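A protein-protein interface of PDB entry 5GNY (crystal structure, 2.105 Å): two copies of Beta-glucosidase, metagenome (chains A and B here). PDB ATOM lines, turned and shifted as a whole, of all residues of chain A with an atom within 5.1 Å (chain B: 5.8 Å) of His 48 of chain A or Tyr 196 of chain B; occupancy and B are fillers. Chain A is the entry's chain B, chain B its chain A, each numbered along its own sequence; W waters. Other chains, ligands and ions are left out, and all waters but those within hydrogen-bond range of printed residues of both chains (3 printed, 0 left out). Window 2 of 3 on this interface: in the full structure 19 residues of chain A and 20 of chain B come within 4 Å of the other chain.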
ATOM      1  N   GLU A  40      20.382  -8.397  34.474  1.00  0.00           N
ATOM      2  CA  GLU A  40      20.446  -8.517  33.023  1.00  0.00           C
ATOM      3  C   GLU A  40      21.898  -8.482  32.569  1.00  0.00           C
ATOM      4  O   GLU A  40      22.652  -7.597  32.971  1.00  0.00           O
ATOM      5  CB  GLU A  40      19.641  -7.394  32.361  1.00  0.00           C
ATOM      6  CG  GLU A  40      19.757  -7.318  30.846  1.00  0.00           C
ATOM      7  CD  GLU A  40      18.887  -6.218  30.254  1.00  0.00           C
ATOM      8  OE1 GLU A  40      17.645  -6.315  30.352  1.00  0.00           O
ATOM      9  OE2 GLU A  40      19.445  -5.248  29.699  1.00  0.00           O
ATOM     10  N   TRP A  43      24.557 -10.838  27.343  1.00  0.00           N
ATOM     11  CA  TRP A  43      24.097 -11.943  26.515  1.00  0.00           C
ATOM     12  C   TRP A  43      22.579 -12.046  26.540  1.00  0.00           C
ATOM     13  O   TRP A  43      21.976 -12.592  25.620  1.00  0.00           O
ATOM     14  CB  TRP A  43      24.750 -13.253  26.955  1.00  0.00           C
ATOM     15  CG  TRP A  43      26.066 -13.453  26.280  1.00  0.00           C
ATOM     16  CD1 TRP A  43      27.304 -13.202  26.797  1.00  0.00           C
ATOM     17  CD2 TRP A  43      26.275 -13.905  24.939  1.00  0.00           C
ATOM     18  NE1 TRP A  43      28.273 -13.490  25.864  1.00  0.00           N
ATOM     19  CE2 TRP A  43      27.666 -13.924  24.715  1.00  0.00           C
ATOM     20  CE3 TRP A  43      25.421 -14.307  23.907  1.00  0.00           C
ATOM     21  CZ2 TRP A  43      28.221 -14.325  23.503  1.00  0.00           C
ATOM     22  CZ3 TRP A  43      25.975 -14.708  22.706  1.00  0.00           C
ATOM     23  CH2 TRP A  43      27.360 -14.715  22.514  1.00  0.00           C
ATOM     24  N   ASP A  44      21.962 -11.504  27.583  1.00  0.00           N
ATOM     25  CA  ASP A  44      20.513 -11.348  27.593  1.00  0.00           C
ATOM     26  C   ASP A  44      20.088 -10.395  26.477  1.00  0.00           C
ATOM     27  O   ASP A  44      19.099 -10.631  25.790  1.00  0.00           O
ATOM     28  CB  ASP A  44      20.026 -10.836  28.950  1.00  0.00           C
ATOM     29  CG  ASP A  44      20.140 -11.884  30.043  1.00  0.00           C
ATOM     30  OD1 ASP A  44      19.881 -13.076  29.762  1.00  0.00           O
ATOM     31  OD2 ASP A  44      20.484 -11.519  31.186  1.00  0.00           O
ATOM     32  N   ARG A  45      20.850  -9.321  26.293  1.00  0.00           N
ATOM     33  CA  ARG A  45      20.569  -8.354  25.236  1.00  0.00           C
ATOM     34  C   ARG A  45      20.899  -8.912  23.856  1.00  0.00           C
ATOM     35  O   ARG A  45      20.063  -8.904  22.952  1.00  0.00           O
ATOM     36  CB  ARG A  45      21.358  -7.064  25.465  1.00  0.00           C
ATOM     37  CG  ARG A  45      20.920  -6.266  26.674  1.00  0.00           C
ATOM     38  CD  ARG A  45      21.768  -5.015  26.825  1.00  0.00           C
ATOM     39  NE  ARG A  45      21.264  -4.143  27.879  1.00  0.00           N
ATOM     40  CZ  ARG A  45      21.864  -3.026  28.279  1.00  0.00           C
ATOM     41  NH1 ARG A  45      23.006  -2.644  27.719  1.00  0.00           N
ATOM     42  NH2 ARG A  45      21.330  -2.301  29.249  1.00  0.00           N
ATOM     43  N   PHE A  46      22.130  -9.390  23.711  1.00  0.00           N
ATOM     44  CA  PHE A  46      22.649  -9.867  22.436  1.00  0.00           C
ATOM     45  C   PHE A  46      21.797 -10.983  21.845  1.00  0.00           C
ATOM     46  O   PHE A  46      21.499 -10.974  20.650  1.00  0.00           O
ATOM     47  CB  PHE A  46      24.091 -10.348  22.614  1.00  0.00           C
ATOM     48  CG  PHE A  46      24.816 -10.626  21.324  1.00  0.00           C
ATOM     49  CD1 PHE A  46      25.466  -9.609  20.644  1.00  0.00           C
ATOM     50  CD2 PHE A  46      24.872 -11.912  20.808  1.00  0.00           C
ATOM     51  CE1 PHE A  46      26.146  -9.864  19.469  1.00  0.00           C
ATOM     52  CE2 PHE A  46      25.550 -12.173  19.632  1.00  0.00           C
ATOM     53  CZ  PHE A  46      26.187 -11.148  18.963  1.00  0.00           C
ATOM     54  N   SER A  47      21.400 -11.936  22.685  1.00  0.00           N
ATOM     55  CA  SER A  47      20.681 -13.117  22.218  1.00  0.00           C
ATOM     56  C   SER A  47      19.256 -12.799  21.768  1.00  0.00           C
ATOM     57  O   SER A  47      18.671 -13.542  20.983  1.00  0.00           O
ATOM     58  CB  SER A  47      20.649 -14.191  23.310  1.00  0.00           C
ATOM     59  OG  SER A  47      19.781 -13.818  24.366  1.00  0.00           O
ATOM     60  N   HIS A  48      18.697 -11.702  22.269  1.00  0.00           N
ATOM     61  CA  HIS A  48      17.323 -11.340  21.935  1.00  0.00           C
ATOM     62  C   HIS A  48      17.262 -10.275  20.847  1.00  0.00           C
ATOM     63  O   HIS A  48      16.212  -9.685  20.596  1.00  0.00           O
ATOM     64  CB  HIS A  48      16.580 -10.870  23.185  1.00  0.00           C
ATOM     65  CG  HIS A  48      16.230 -11.982  24.124  1.00  0.00           C
ATOM     66  ND1 HIS A  48      15.028 -12.655  24.061  1.00  0.00           N
ATOM     67  CD2 HIS A  48      16.929 -12.554  25.132  1.00  0.00           C
ATOM     68  CE1 HIS A  48      14.999 -13.586  24.996  1.00  0.00           C
ATOM     69  NE2 HIS A  48      16.141 -13.547  25.661  1.00  0.00           N
ATOM     70  N   THR A  49      18.397 -10.042  20.200  1.00  0.00           N
ATOM     71  CA  THR A  49      18.470  -9.128  19.071  1.00  0.00           C
ATOM     72  C   THR A  49      18.491  -9.945  17.786  1.00  0.00           C
ATOM     73  O   THR A  49      19.380 -10.775  17.595  1.00  0.00           O
ATOM     74  CB  THR A  49      19.717  -8.229  19.151  1.00  0.00           C
ATOM     75  OG1 THR A  49      19.741  -7.560  20.417  1.00  0.00           O
ATOM     76  CG2 THR A  49      19.718  -7.195  18.029  1.00  0.00           C
ATOM     77  N   PRO A  50      17.503  -9.724  16.907  1.00  0.00           N
ATOM     78  CA  PRO A  50      17.350 -10.539  15.694  1.00  0.00           C
ATOM     79  C   PRO A  50      18.602 -10.556  14.823  1.00  0.00           C
ATOM     80  O   PRO A  50      19.227  -9.515  14.625  1.00  0.00           O
ATOM     81  CB  PRO A  50      16.188  -9.860  14.957  1.00  0.00           C
ATOM     82  CG  PRO A  50      16.130  -8.475  15.516  1.00  0.00           C
ATOM     83  CD  PRO A  50      16.534  -8.618  16.952  1.00  0.00           C
ATOM     84  N   THR A  58      18.304 -18.659  22.144  1.00  0.00           N
ATOM     85  CA  THR A  58      18.783 -17.868  23.272  1.00  0.00           C
ATOM     86  C   THR A  58      19.119 -18.786  24.439  1.00  0.00           C
ATOM     87  O   THR A  58      18.894 -19.995  24.374  1.00  0.00           O
ATOM     88  CB  THR A  58      17.751 -16.823  23.745  1.00  0.00           C
ATOM     89  OG1 THR A  58      16.765 -17.458  24.568  1.00  0.00           O
ATOM     90  CG2 THR A  58      17.081 -16.127  22.563  1.00  0.00           C
ATOM     91  N   ASP A  60      17.708 -18.527  27.357  1.00  0.00           N
ATOM     92  CA  ASP A  60      16.595 -18.376  28.289  1.00  0.00           C
ATOM     93  C   ASP A  60      16.313 -19.659  29.063  1.00  0.00           C
ATOM     94  O   ASP A  60      16.030 -19.620  30.261  1.00  0.00           O
ATOM     95  CB  ASP A  60      15.327 -17.937  27.556  1.00  0.00           C
ATOM     96  CG  ASP A  60      15.372 -16.485  27.135  1.00  0.00           C
ATOM     97  OD1 ASP A  60      16.381 -15.809  27.423  1.00  0.00           O
ATOM     98  OD2 ASP A  60      14.387 -16.015  26.532  1.00  0.00           O
ATOM     99  N   LEU B 143      24.897   5.554  26.722  1.00  0.00           N
ATOM    100  CA  LEU B 143      24.309   4.543  27.596  1.00  0.00           C
ATOM    101  C   LEU B 143      24.574   4.853  29.072  1.00  0.00           C
ATOM    102  O   LEU B 143      23.896   4.333  29.960  1.00  0.00           O
ATOM    103  CB  LEU B 143      24.850   3.154  27.254  1.00  0.00           C
ATOM    104  CG  LEU B 143      24.667   2.682  25.810  1.00  0.00           C
ATOM    105  CD1 LEU B 143      25.191   1.268  25.650  1.00  0.00           C
ATOM    106  CD2 LEU B 143      23.207   2.779  25.398  1.00  0.00           C
ATOM    107  N   SER B 194      21.268  -2.701  18.657  1.00  0.00           N
ATOM    108  CA  SER B 194      20.562  -3.222  19.819  1.00  0.00           C
ATOM    109  C   SER B 194      19.370  -2.349  20.185  1.00  0.00           C
ATOM    110  O   SER B 194      19.512  -1.136  20.354  1.00  0.00           O
ATOM    111  CB  SER B 194      21.511  -3.323  21.015  1.00  0.00           C
ATOM    112  OG  SER B 194      20.794  -3.556  22.215  1.00  0.00           O
ATOM    113  N   ALA B 195      18.198  -2.960  20.316  1.00  0.00           N
ATOM    114  CA  ALA B 195      17.015  -2.221  20.745  1.00  0.00           C
ATOM    115  C   ALA B 195      17.123  -1.837  22.224  1.00  0.00           C
ATOM    116  O   ALA B 195      16.628  -0.787  22.640  1.00  0.00           O
ATOM    117  CB  ALA B 195      15.757  -3.033  20.495  1.00  0.00           C
ATOM    118  N   TYR B 196      17.775  -2.690  23.010  1.00  0.00           N
ATOM    119  CA  TYR B 196      17.984  -2.413  24.429  1.00  0.00           C
ATOM    120  C   TYR B 196      18.813  -1.148  24.607  1.00  0.00           C
ATOM    121  O   TYR B 196      18.480  -0.286  25.425  1.00  0.00           O
ATOM    122  CB  TYR B 196      18.666  -3.594  25.122  1.00  0.00           C
ATOM    123  CG  TYR B 196      17.845  -4.862  25.113  1.00  0.00           C
ATOM    124  CD1 TYR B 196      17.906  -5.744  24.042  1.00  0.00           C
ATOM    125  CD2 TYR B 196      17.005  -5.177  26.176  1.00  0.00           C
ATOM    126  CE1 TYR B 196      17.159  -6.903  24.027  1.00  0.00           C
ATOM    127  CE2 TYR B 196      16.252  -6.334  26.172  1.00  0.00           C
ATOM    128  CZ  TYR B 196      16.333  -7.193  25.094  1.00  0.00           C
ATOM    129  OH  TYR B 196      15.589  -8.348  25.078  1.00  0.00           O
ATOM    130  N   GLU B 197      19.882  -1.033  23.827  1.00  0.00           N
ATOM    131  CA  GLU B 197      20.743   0.139  23.892  1.00  0.00           C
ATOM    132  C   GLU B 197      20.075   1.367  23.288  1.00  0.00           C
ATOM    133  O   GLU B 197      20.263   2.482  23.772  1.00  0.00           O
ATOM    134  CB  GLU B 197      22.074  -0.132  23.191  1.00  0.00           C
ATOM    135  CG  GLU B 197      22.915  -1.195  23.873  1.00  0.00           C
ATOM    136  CD  GLU B 197      24.301  -1.310  23.276  1.00  0.00           C
ATOM    137  OE1 GLU B 197      24.639  -0.497  22.390  1.00  0.00           O
ATOM    138  OE2 GLU B 197      25.054  -2.216  23.693  1.00  0.00           O
ATOM    139  N   ALA B 198      19.291   1.160  22.235  1.00  0.00           N
ATOM    140  CA  ALA B 198      18.587   2.261  21.584  1.00  0.00           C
ATOM    141  C   ALA B 198      17.634   2.968  22.551  1.00  0.00           C
ATOM    142  O   ALA B 198      17.583   4.197  22.600  1.00  0.00           O
ATOM    143  CB  ALA B 198      17.828   1.756  20.371  1.00  0.00           C
ATOM    144  N   VAL B 199      16.881   2.182  23.313  1.00  0.00           N
ATOM    145  CA  VAL B 199      15.931   2.720  24.278  1.00  0.00           C
ATOM    146  C   VAL B 199      16.648   3.555  25.335  1.00  0.00           C
ATOM    147  O   VAL B 199      16.215   4.658  25.667  1.00  0.00           O
ATOM    148  CB  VAL B 199      15.128   1.593  24.962  1.00  0.00           C
ATOM    149  CG1 VAL B 199      14.347   2.129  26.158  1.00  0.00           C
ATOM    150  CG2 VAL B 199      14.193   0.932  23.961  1.00  0.00           C
ATOM    151  N   ILE B 200      17.758   3.029  25.841  1.00  0.00           N
ATOM    152  CA  ILE B 200      18.526   3.705  26.877  1.00  0.00           C
ATOM    153  C   ILE B 200      19.221   4.954  26.333  1.00  0.00           C
ATOM    154  O   ILE B 200      19.204   6.013  26.972  1.00  0.00           O
ATOM    155  CB  ILE B 200      19.567   2.755  27.498  1.00  0.00           C
ATOM    156  CG1 ILE B 200      18.853   1.635  28.258  1.00  0.00           C
ATOM    157  CG2 ILE B 200      20.498   3.507  28.441  1.00  0.00           C
ATOM    158  CD1 ILE B 200      19.756   0.503  28.663  1.00  0.00           C
ATOM    159  N   ALA B 201      19.818   4.828  25.152  1.00  0.00           N
ATOM    160  CA  ALA B 201      20.507   5.944  24.513  1.00  0.00           C
ATOM    161  C   ALA B 201      19.545   7.092  24.251  1.00  0.00           C
ATOM    162  O   ALA B 201      19.884   8.253  24.464  1.00  0.00           O
ATOM    163  CB  ALA B 201      21.165   5.496  23.204  1.00  0.00           C
ATOM    164  N   ALA B 276      10.291  -6.235  24.659  1.00  0.00           N
ATOM    165  CA  ALA B 276      11.026  -6.562  25.881  1.00  0.00           C
ATOM    166  C   ALA B 276      12.185  -5.604  26.147  1.00  0.00           C
ATOM    167  O   ALA B 276      12.703  -5.542  27.261  1.00  0.00           O
ATOM    168  CB  ALA B 276      11.539  -7.990  25.812  1.00  0.00           C
ATOM    169  N   ALA B 277      12.594  -4.867  25.121  1.00  0.00           N
ATOM    170  CA  ALA B 277      13.673  -3.900  25.262  1.00  0.00           C
ATOM    171  C   ALA B 277      13.169  -2.593  25.868  1.00  0.00           C
ATOM    172  O   ALA B 277      13.961  -1.739  26.265  1.00  0.00           O
ATOM    173  CB  ALA B 277      14.329  -3.637  23.914  1.00  0.00           C
HETATM  174  O   HOH W   1      24.853  -4.240  25.622  1.00  0.00           O
HETATM  175  O   HOH W   2      21.269  -6.239  22.305  1.00  0.00           O
HETATM  176  O   HOH W   3      17.517  -5.715  20.571  1.00  0.00           O
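Of the printed residues of chain B, Arg 45 of chain A touches Tyr 196 (3.7 Å) and Ile 200 (3.3 Å). Printed residues of chain B within 4 Å of His 48 of chain A: Tyr 196. Ser 194 of chain B touches none of the printed residues of chain A. Tyr 196 of chain B touches two residues of chain A. Glu 197 of chain B touches none of the printed residues of chain A. Printed residues of chain A within 4 Å of Ile 200 of chain B: Arg 45. The nearest printed residue of chain B that does not touch Arg 45 of chain A is Glu 197 of chain B (4.1 Å).
OE2 of Glu 40 of chain A lies within salt-bridge range of NE of Arg 45 of chain A, 2.8 Å away. O of Arg 45 of chain A is in hydrogen-bond range of OG1 of Thr 49 of chain A, at 2.9 Å. A ring nitrogen (NE2) of His 48 of chain A is in hydrogen-bond range of the side-chain carboxylate (OD1) of Asp 60 of chain A, at 2.9 Å. The backbone NH (N) of Tyr 196 of chain B is in hydrogen-bond range of the side-chain hydroxyl (OG) of Ser 194 of chain B (3.2 Å).
Water W2 lies within hydrogen-bond range of the side-chain hydroxyl (OG) of Ser 194 of chain B (2.7 Å), the side-chain hydroxyl (OG1) of Thr 49 of chain A (2.8 Å) and the backbone carbonyl oxygen (O) of Arg 45 of chain A (3.0 Å). Water W1 lies within hydrogen-bond range of OE2 of Glu 197 of chain B (2.8 Å) and NH1 of Arg 45 of chain A (3.2 Å). Water W3 lies within hydrogen-bond range of the backbone NH of Ala 195 of chain B and the side-chain hydroxyl of Thr 49 of chain A.
No position is printed for both chains.
Printed residues of chain A that touch a printed residue of chain B: Arg 45 and His 48. Hydrophobic or aromatic side chains of chain A that line the printed part of chain B: His 48. Hydrophobic or aromatic side chains of chain B within 4 Å of the printed part of chain A: Tyr 196 and Ile 200.
Arg 45 of chain A touches Tyr 196 of chain B (O to CE1, 3.7 Å). Ile 200 of chain B touches Arg 45 of chain A. Tyr 196 of chain B touches His 48 of chain A.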
